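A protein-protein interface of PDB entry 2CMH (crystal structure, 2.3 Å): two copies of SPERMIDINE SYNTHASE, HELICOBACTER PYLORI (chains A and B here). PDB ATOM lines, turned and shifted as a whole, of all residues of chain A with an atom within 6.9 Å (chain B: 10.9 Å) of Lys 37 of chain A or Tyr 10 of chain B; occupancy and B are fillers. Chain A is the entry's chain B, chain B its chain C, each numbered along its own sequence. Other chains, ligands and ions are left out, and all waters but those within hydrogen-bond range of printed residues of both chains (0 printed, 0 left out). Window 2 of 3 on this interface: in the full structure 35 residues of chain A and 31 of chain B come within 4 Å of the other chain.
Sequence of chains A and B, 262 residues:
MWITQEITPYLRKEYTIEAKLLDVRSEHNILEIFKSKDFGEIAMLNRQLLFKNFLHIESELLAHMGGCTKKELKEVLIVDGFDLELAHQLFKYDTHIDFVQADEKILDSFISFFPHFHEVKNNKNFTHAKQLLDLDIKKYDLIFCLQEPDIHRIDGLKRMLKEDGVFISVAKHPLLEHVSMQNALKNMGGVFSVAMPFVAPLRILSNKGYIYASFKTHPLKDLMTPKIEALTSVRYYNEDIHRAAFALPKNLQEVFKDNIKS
Hydrophobic or aromatic side chains of chain B within 4 Å of the printed part of chain A: Tyr 10 and Leu 11. Among the printed residues, no Asp or Glu carboxylate lies within 4 Å of a Lys or Arg side-chain nitrogen of the other chain.
The guanidinium group (NH1) of Arg 12 of chain B lies within salt-bridge range of the side-chain carboxylate (OE1) of Glu 6 of chain B, at 3.4 Å.
The backbone NH (N) of Glu 14 of chain A sits at hydrogen-bond distance from the backbone carbonyl oxygen (O) of Arg 12 of chain B. N of Thr 16 of chain A lies within hydrogen-bond range of O of Tyr 10 of chain B (3.1 Å). OH of Tyr 10 of chain B lies close to NZ of Lys 37 of chain A. The backbone carbonyl oxygen of Tyr 10 of chain B lies close to the backbone carbonyl oxygen of Glu 14 of chain A (3.4 Å).
No position is printed for both chains. Of the 9 pairs that touch across the chains among the printed residues, none has its exchanged pair printed and touching as well.
Of chain B, only Tyr 10 comes within 4 Å of Lys 37 of chain A. Tyr 10 of chain B touches just these residues of chain A: Glu 14, Tyr 15, Thr 16, Lys 37 and Asp 38. No residue of chain B comes within 4 Å of Gly 40 of chain A. Of the printed residues of chain B, Tyr 15 of chain A touches Tyr 10 and Leu 11. Of the printed residues of chain A, Arg 12 of chain B touches Trp 2 (3.3 Å) and Glu 14 (2.8 Å). Ile 7 of chain B touches none of the printed residues of chain A. The nearest residue of chain B that does not touch Lys 37 of chain A is Pro 9 of chain B (7.8 Å). The nearest residue of chain A that does not touch Tyr 10 of chain B is Trp 2 of chain A (4.3 Å). The nearest printed residue of chain A that does not touch Leu 11 of chain B is Trp 2 of chain A (4.6 Å).
Trp 2 of chain A touches Arg 12 of chain B. Leu 11 of chain B touches Glu 14 of chain A. CA of Tyr 15 of chain A touches O of Tyr 10 of chain B, 3.4 Å away. Tyr 15 of chain A touches Leu 11 of chain B (CE1 to CD1, 3.7 Å). OD1 of Asp 38 of chain A touches CD2 of Tyr 10 of chain B, 3.0 Å away.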
ATOM      1  N   TRP A   2     -13.985 -27.304 -13.838  1.00  0.00           N
ATOM      2  CA  TRP A   2     -14.663 -27.043 -15.094  1.00  0.00           C
ATOM      3  C   TRP A   2     -13.782 -27.214 -16.332  1.00  0.00           C
ATOM      4  O   TRP A   2     -12.556 -27.220 -16.258  1.00  0.00           O
ATOM      5  CB  TRP A   2     -15.223 -25.612 -15.103  1.00  0.00           C
ATOM      6  CG  TRP A   2     -16.161 -25.266 -13.979  1.00  0.00           C
ATOM      7  CD1 TRP A   2     -15.864 -25.195 -12.643  1.00  0.00           C
ATOM      8  CD2 TRP A   2     -17.540 -24.901 -14.101  1.00  0.00           C
ATOM      9  NE1 TRP A   2     -16.975 -24.801 -11.931  1.00  0.00           N
ATOM     10  CE2 TRP A   2     -18.016 -24.610 -12.803  1.00  0.00           C
ATOM     11  CE3 TRP A   2     -18.421 -24.777 -15.188  1.00  0.00           C
ATOM     12  CZ2 TRP A   2     -19.336 -24.217 -12.561  1.00  0.00           C
ATOM     13  CZ3 TRP A   2     -19.730 -24.385 -14.948  1.00  0.00           C
ATOM     14  CH2 TRP A   2     -20.174 -24.104 -13.647  1.00  0.00           C
ATOM     15  N   GLU A  14     -19.610 -23.881 -20.394  1.00  0.00           N
ATOM     16  CA  GLU A  14     -18.770 -24.377 -19.317  1.00  0.00           C
ATOM     17  C   GLU A  14     -19.435 -25.472 -18.503  1.00  0.00           C
ATOM     18  O   GLU A  14     -20.467 -25.265 -17.860  1.00  0.00           O
ATOM     19  CB  GLU A  14     -18.322 -23.216 -18.432  1.00  0.00           C
ATOM     20  CG  GLU A  14     -17.759 -22.068 -19.249  1.00  0.00           C
ATOM     21  CD  GLU A  14     -16.906 -21.138 -18.438  1.00  0.00           C
ATOM     22  OE1 GLU A  14     -17.360 -20.708 -17.353  1.00  0.00           O
ATOM     23  OE2 GLU A  14     -15.780 -20.839 -18.901  1.00  0.00           O
ATOM     24  N   TYR A  15     -18.823 -26.649 -18.558  1.00  0.00           N
ATOM     25  CA  TYR A  15     -19.313 -27.828 -17.869  1.00  0.00           C
ATOM     26  C   TYR A  15     -18.551 -28.131 -16.597  1.00  0.00           C
ATOM     27  O   TYR A  15     -17.322 -28.246 -16.599  1.00  0.00           O
ATOM     28  CB  TYR A  15     -19.202 -29.039 -18.784  1.00  0.00           C
ATOM     29  CG  TYR A  15     -20.041 -28.949 -20.022  1.00  0.00           C
ATOM     30  CD1 TYR A  15     -21.376 -29.347 -20.009  1.00  0.00           C
ATOM     31  CD2 TYR A  15     -19.500 -28.487 -21.217  1.00  0.00           C
ATOM     32  CE1 TYR A  15     -22.149 -29.292 -21.159  1.00  0.00           C
ATOM     33  CE2 TYR A  15     -20.265 -28.427 -22.371  1.00  0.00           C
ATOM     34  CZ  TYR A  15     -21.587 -28.835 -22.335  1.00  0.00           C
ATOM     35  OH  TYR A  15     -22.343 -28.819 -23.481  1.00  0.00           O
ATOM     36  N   THR A  16     -19.294 -28.275 -15.512  1.00  0.00           N
ATOM     37  CA  THR A  16     -18.693 -28.633 -14.245  1.00  0.00           C
ATOM     38  C   THR A  16     -18.368 -30.117 -14.420  1.00  0.00           C
ATOM     39  O   THR A  16     -19.190 -30.880 -14.916  1.00  0.00           O
ATOM     40  CB  THR A  16     -19.697 -28.418 -13.109  1.00  0.00           C
ATOM     41  OG1 THR A  16     -20.021 -27.023 -13.030  1.00  0.00           O
ATOM     42  CG2 THR A  16     -19.127 -28.870 -11.789  1.00  0.00           C
ATOM     43  N   ILE A  17     -17.147 -30.498 -14.054  1.00  0.00           N
ATOM     44  CA  ILE A  17     -16.664 -31.879 -14.160  1.00  0.00           C
ATOM     45  C   ILE A  17     -16.238 -32.392 -12.780  1.00  0.00           C
ATOM     46  O   ILE A  17     -15.755 -31.623 -11.946  1.00  0.00           O
ATOM     47  CB  ILE A  17     -15.467 -31.965 -15.159  1.00  0.00           C
ATOM     48  CG1 ILE A  17     -15.958 -32.431 -16.526  1.00  0.00           C
ATOM     49  CG2 ILE A  17     -14.397 -32.919 -14.664  1.00  0.00           C
ATOM     50  CD1 ILE A  17     -16.819 -31.433 -17.238  1.00  0.00           C
ATOM     51  N   GLU A  18     -16.423 -33.686 -12.534  1.00  0.00           N
ATOM     52  CA  GLU A  18     -16.045 -34.262 -11.244  1.00  0.00           C
ATOM     53  C   GLU A  18     -14.660 -34.893 -11.286  1.00  0.00           C
ATOM     54  O   GLU A  18     -13.960 -34.967 -10.273  1.00  0.00           O
ATOM     55  CB  GLU A  18     -17.042 -35.338 -10.816  1.00  0.00           C
ATOM     56  CG  GLU A  18     -18.463 -34.859 -10.597  1.00  0.00           C
ATOM     57  CD  GLU A  18     -19.331 -35.916  -9.936  1.00  0.00           C
ATOM     58  OE1 GLU A  18     -20.567 -35.730  -9.897  1.00  0.00           O
ATOM     59  OE2 GLU A  18     -18.781 -36.927  -9.437  1.00  0.00           O
ATOM     60  N   LYS A  35     -15.761 -37.106 -16.249  1.00  0.00           N
ATOM     61  CA  LYS A  35     -16.974 -37.611 -15.610  1.00  0.00           C
ATOM     62  C   LYS A  35     -17.813 -36.407 -15.196  1.00  0.00           C
ATOM     63  O   LYS A  35     -17.338 -35.534 -14.470  1.00  0.00           O
ATOM     64  CB  LYS A  35     -16.643 -38.442 -14.368  1.00  0.00           C
ATOM     65  CG  LYS A  35     -17.878 -39.034 -13.680  1.00  0.00           C
ATOM     66  CD  LYS A  35     -17.542 -39.697 -12.348  1.00  0.00           C
ATOM     67  CE  LYS A  35     -16.551 -40.850 -12.504  1.00  0.00           C
ATOM     68  NZ  LYS A  35     -17.057 -42.022 -13.311  1.00  0.00           N
ATOM     69  N   SER A  36     -19.049 -36.349 -15.680  1.00  0.00           N
ATOM     70  CA  SER A  36     -19.965 -35.266 -15.323  1.00  0.00           C
ATOM     71  C   SER A  36     -21.095 -35.897 -14.525  1.00  0.00           C
ATOM     72  O   SER A  36     -21.515 -37.012 -14.831  1.00  0.00           O
ATOM     73  CB  SER A  36     -20.534 -34.601 -16.582  1.00  0.00           C
ATOM     74  OG  SER A  36     -21.352 -33.489 -16.261  1.00  0.00           O
ATOM     75  N   LYS A  37     -21.587 -35.198 -13.509  1.00  0.00           N
ATOM     76  CA  LYS A  37     -22.676 -35.729 -12.702  1.00  0.00           C
ATOM     77  C   LYS A  37     -24.012 -35.738 -13.446  1.00  0.00           C
ATOM     78  O   LYS A  37     -25.010 -36.228 -12.919  1.00  0.00           O
ATOM     79  CB  LYS A  37     -22.847 -34.911 -11.420  1.00  0.00           C
ATOM     80  CG  LYS A  37     -24.010 -35.394 -10.551  1.00  0.00           C
ATOM     81  CD  LYS A  37     -24.358 -34.401  -9.458  1.00  0.00           C
ATOM     82  CE  LYS A  37     -25.730 -34.699  -8.857  1.00  0.00           C
ATOM     83  NZ  LYS A  37     -26.177 -33.644  -7.898  1.00  0.00           N
ATOM     84  N   ASP A  38     -24.047 -35.206 -14.666  1.00  0.00           N
ATOM     85  CA  ASP A  38     -25.314 -35.164 -15.389  1.00  0.00           C
ATOM     86  C   ASP A  38     -25.325 -35.755 -16.787  1.00  0.00           C
ATOM     87  O   ASP A  38     -26.245 -36.495 -17.148  1.00  0.00           O
ATOM     88  CB  ASP A  38     -25.821 -33.722 -15.473  1.00  0.00           C
ATOM     89  CG  ASP A  38     -25.756 -32.998 -14.140  1.00  0.00           C
ATOM     90  OD1 ASP A  38     -26.756 -32.348 -13.780  1.00  0.00           O
ATOM     91  OD2 ASP A  38     -24.699 -33.068 -13.472  1.00  0.00           O
ATOM     92  N   PHE A  39     -24.312 -35.421 -17.575  1.00  0.00           N
ATOM     93  CA  PHE A  39     -24.223 -35.886 -18.951  1.00  0.00           C
ATOM     94  C   PHE A  39     -23.422 -37.183 -19.044  1.00  0.00           C
ATOM     95  O   PHE A  39     -22.994 -37.604 -20.123  1.00  0.00           O
ATOM     96  CB  PHE A  39     -23.594 -34.782 -19.805  1.00  0.00           C
ATOM     97  CG  PHE A  39     -24.142 -33.411 -19.514  1.00  0.00           C
ATOM     98  CD1 PHE A  39     -23.704 -32.691 -18.404  1.00  0.00           C
ATOM     99  CD2 PHE A  39     -25.138 -32.863 -20.313  1.00  0.00           C
ATOM    100  CE1 PHE A  39     -24.255 -31.442 -18.091  1.00  0.00           C
ATOM    101  CE2 PHE A  39     -25.694 -31.625 -20.009  1.00  0.00           C
ATOM    102  CZ  PHE A  39     -25.255 -30.912 -18.899  1.00  0.00           C
ATOM    103  N   GLY A  40     -23.251 -37.828 -17.898  1.00  0.00           N
ATOM    104  CA  GLY A  40     -22.490 -39.062 -17.854  1.00  0.00           C
ATOM    105  C   GLY A  40     -21.055 -38.668 -18.104  1.00  0.00           C
ATOM    106  O   GLY A  40     -20.591 -37.664 -17.568  1.00  0.00           O
ATOM    107  N   GLN B   5     -23.984 -16.540 -18.077  1.00  0.00           N
ATOM    108  CA  GLN B   5     -25.327 -16.951 -17.687  1.00  0.00           C
ATOM    109  C   GLN B   5     -25.349 -18.431 -17.329  1.00  0.00           C
ATOM    110  O   GLN B   5     -24.763 -19.261 -18.037  1.00  0.00           O
ATOM    111  CB  GLN B   5     -26.318 -16.704 -18.817  1.00  0.00           C
ATOM    112  CG  GLN B   5     -26.063 -17.545 -20.059  1.00  0.00           C
ATOM    113  CD  GLN B   5     -27.305 -17.676 -20.910  1.00  0.00           C
ATOM    114  OE1 GLN B   5     -27.231 -18.003 -22.092  1.00  0.00           O
ATOM    115  NE2 GLN B   5     -28.464 -17.438 -20.303  1.00  0.00           N
ATOM    116  N   GLU B   6     -26.026 -18.764 -16.235  1.00  0.00           N
ATOM    117  CA  GLU B   6     -26.113 -20.157 -15.823  1.00  0.00           C
ATOM    118  C   GLU B   6     -27.333 -20.724 -16.522  1.00  0.00           C
ATOM    119  O   GLU B   6     -28.454 -20.296 -16.248  1.00  0.00           O
ATOM    120  CB  GLU B   6     -26.327 -20.294 -14.312  1.00  0.00           C
ATOM    121  CG  GLU B   6     -25.632 -19.277 -13.425  1.00  0.00           C
ATOM    122  CD  GLU B   6     -25.936 -19.508 -11.947  1.00  0.00           C
ATOM    123  OE1 GLU B   6     -25.423 -20.492 -11.370  1.00  0.00           O
ATOM    124  OE2 GLU B   6     -26.702 -18.708 -11.363  1.00  0.00           O
ATOM    125  N   ILE B   7     -27.136 -21.662 -17.439  1.00  0.00           N
ATOM    126  CA  ILE B   7     -28.289 -22.251 -18.101  1.00  0.00           C
ATOM    127  C   ILE B   7     -28.631 -23.533 -17.340  1.00  0.00           C
ATOM    128  O   ILE B   7     -29.726 -24.079 -17.474  1.00  0.00           O
ATOM    129  CB  ILE B   7     -28.020 -22.540 -19.617  1.00  0.00           C
ATOM    130  CG1 ILE B   7     -27.068 -23.723 -19.795  1.00  0.00           C
ATOM    131  CG2 ILE B   7     -27.473 -21.292 -20.299  1.00  0.00           C
ATOM    132  CD1 ILE B   7     -27.766 -25.083 -19.768  1.00  0.00           C
ATOM    133  N   THR B   8     -27.671 -23.988 -16.534  1.00  0.00           N
ATOM    134  CA  THR B   8     -27.811 -25.183 -15.700  1.00  0.00           C
ATOM    135  C   THR B   8     -26.852 -25.096 -14.506  1.00  0.00           C
ATOM    136  O   THR B   8     -25.833 -24.404 -14.564  1.00  0.00           O
ATOM    137  CB  THR B   8     -27.529 -26.481 -16.529  1.00  0.00           C
ATOM    138  OG1 THR B   8     -28.762 -27.164 -16.792  1.00  0.00           O
ATOM    139  CG2 THR B   8     -26.588 -27.421 -15.810  1.00  0.00           C
ATOM    140  N   PRO B   9     -27.170 -25.796 -13.401  1.00  0.00           N
ATOM    141  CA  PRO B   9     -26.286 -25.751 -12.227  1.00  0.00           C
ATOM    142  C   PRO B   9     -24.893 -26.284 -12.571  1.00  0.00           C
ATOM    143  O   PRO B   9     -23.918 -26.024 -11.866  1.00  0.00           O
ATOM    144  CB  PRO B   9     -27.003 -26.648 -11.215  1.00  0.00           C
ATOM    145  CG  PRO B   9     -28.452 -26.546 -11.616  1.00  0.00           C
ATOM    146  CD  PRO B   9     -28.363 -26.617 -13.125  1.00  0.00           C
ATOM    147  N   TYR B  10     -24.824 -27.037 -13.664  1.00  0.00           N
ATOM    148  CA  TYR B  10     -23.587 -27.637 -14.140  1.00  0.00           C
ATOM    149  C   TYR B  10     -23.198 -27.111 -15.521  1.00  0.00           C
ATOM    150  O   TYR B  10     -22.263 -27.613 -16.140  1.00  0.00           O
ATOM    151  CB  TYR B  10     -23.736 -29.167 -14.183  1.00  0.00           C
ATOM    152  CG  TYR B  10     -23.867 -29.811 -12.814  1.00  0.00           C
ATOM    153  CD1 TYR B  10     -22.761 -29.927 -11.970  1.00  0.00           C
ATOM    154  CD2 TYR B  10     -25.098 -30.278 -12.352  1.00  0.00           C
ATOM    155  CE1 TYR B  10     -22.877 -30.489 -10.695  1.00  0.00           C
ATOM    156  CE2 TYR B  10     -25.226 -30.847 -11.074  1.00  0.00           C
ATOM    157  CZ  TYR B  10     -24.110 -30.945 -10.249  1.00  0.00           C
ATOM    158  OH  TYR B  10     -24.220 -31.476  -8.980  1.00  0.00           O
ATOM    159  N   LEU B  11     -23.915 -26.103 -16.010  1.00  0.00           N
ATOM    160  CA  LEU B  11     -23.602 -25.533 -17.321  1.00  0.00           C
ATOM    161  C   LEU B  11     -23.843 -24.029 -17.411  1.00  0.00           C
ATOM    162  O   LEU B  11     -24.931 -23.543 -17.114  1.00  0.00           O
ATOM    163  CB  LEU B  11     -24.403 -26.239 -18.419  1.00  0.00           C
ATOM    164  CG  LEU B  11     -24.232 -25.705 -19.848  1.00  0.00           C
ATOM    165  CD1 LEU B  11     -22.776 -25.748 -20.276  1.00  0.00           C
ATOM    166  CD2 LEU B  11     -25.083 -26.539 -20.794  1.00  0.00           C
ATOM    167  N   ARG B  12     -22.808 -23.302 -17.826  1.00  0.00           N
ATOM    168  CA  ARG B  12     -22.885 -21.851 -17.986  1.00  0.00           C
ATOM    169  C   ARG B  12     -22.510 -21.492 -19.411  1.00  0.00           C
ATOM    170  O   ARG B  12     -21.972 -22.306 -20.153  1.00  0.00           O
ATOM    171  CB  ARG B  12     -21.886 -21.125 -17.083  1.00  0.00           C
ATOM    172  CG  ARG B  12     -22.016 -21.290 -15.594  1.00  0.00           C
ATOM    173  CD  ARG B  12     -20.904 -20.465 -14.976  1.00  0.00           C
ATOM    174  NE  ARG B  12     -20.609 -20.798 -13.588  1.00  0.00           N
ATOM    175  CZ  ARG B  12     -21.354 -20.442 -12.550  1.00  0.00           C
ATOM    176  NH1 ARG B  12     -22.459 -19.735 -12.736  1.00  0.00           N
ATOM    177  NH2 ARG B  12     -20.982 -20.781 -11.322  1.00  0.00           N
ATOM    178  N   LYS B  13     -22.778 -20.250 -19.771  1.00  0.00           N
ATOM    179  CA  LYS B  13     -22.428 -19.748 -21.084  1.00  0.00           C
ATOM    180  C   LYS B  13     -21.645 -18.473 -20.860  1.00  0.00           C
ATOM    181  O   LYS B  13     -21.971 -17.688 -19.973  1.00  0.00           O
ATOM    182  CB  LYS B  13     -23.676 -19.441 -21.922  1.00  0.00           C
ATOM    183  CG  LYS B  13     -24.427 -20.656 -22.437  1.00  0.00           C
ATOM    184  CD  LYS B  13     -25.501 -20.228 -23.421  1.00  0.00           C
ATOM    185  CE  LYS B  13     -26.288 -21.415 -23.938  1.00  0.00           C
ATOM    186  NZ  LYS B  13     -27.357 -20.999 -24.886  1.00  0.00           N
ATOM    187  N   LEU B 176     -33.458 -31.129 -22.126  1.00  0.00           N
ATOM    188  CA  LEU B 176     -32.496 -30.742 -21.110  1.00  0.00           C
ATOM    189  C   LEU B 176     -33.095 -30.829 -19.706  1.00  0.00           C
ATOM    190  O   LEU B 176     -32.428 -31.228 -18.761  1.00  0.00           O
ATOM    191  CB  LEU B 176     -32.034 -29.313 -21.385  1.00  0.00           C
ATOM    192  CG  LEU B 176     -30.649 -28.935 -20.865  1.00  0.00           C
ATOM    193  CD1 LEU B 176     -29.625 -29.935 -21.417  1.00  0.00           C
ATOM    194  CD2 LEU B 176     -30.297 -27.508 -21.298  1.00  0.00           C
ATOM    195  N   GLU B 177     -34.363 -30.453 -19.595  1.00  0.00           N
ATOM    196  CA  GLU B 177     -35.077 -30.454 -18.330  1.00  0.00           C
ATOM    197  C   GLU B 177     -36.471 -31.062 -18.502  1.00  0.00           C
ATOM    198  O   GLU B 177     -37.484 -30.375 -18.324  1.00  0.00           O
ATOM    199  CB  GLU B 177     -35.218 -29.021 -17.806  1.00  0.00           C
ATOM    200  CG  GLU B 177     -33.923 -28.336 -17.390  1.00  0.00           C
ATOM    201  CD  GLU B 177     -34.181 -27.077 -16.571  1.00  0.00           C
ATOM    202  OE1 GLU B 177     -34.767 -27.183 -15.466  1.00  0.00           O
ATOM    203  OE2 GLU B 177     -33.801 -25.979 -17.034  1.00  0.00           O
ATOM    204  N   ASN B 207     -32.345 -22.505 -23.147  1.00  0.00           N
ATOM    205  CA  ASN B 207     -32.919 -23.638 -22.435  1.00  0.00           C
ATOM    206  C   ASN B 207     -34.366 -23.208 -22.233  1.00  0.00           C
ATOM    207  O   ASN B 207     -34.777 -22.848 -21.128  1.00  0.00           O
ATOM    208  CB  ASN B 207     -32.238 -23.815 -21.089  1.00  0.00           C
ATOM    209  CG  ASN B 207     -32.867 -24.908 -20.242  1.00  0.00           C
ATOM    210  OD1 ASN B 207     -32.356 -25.215 -19.167  1.00  0.00           O
ATOM    211  ND2 ASN B 207     -33.963 -25.496 -20.711  1.00  0.00           N
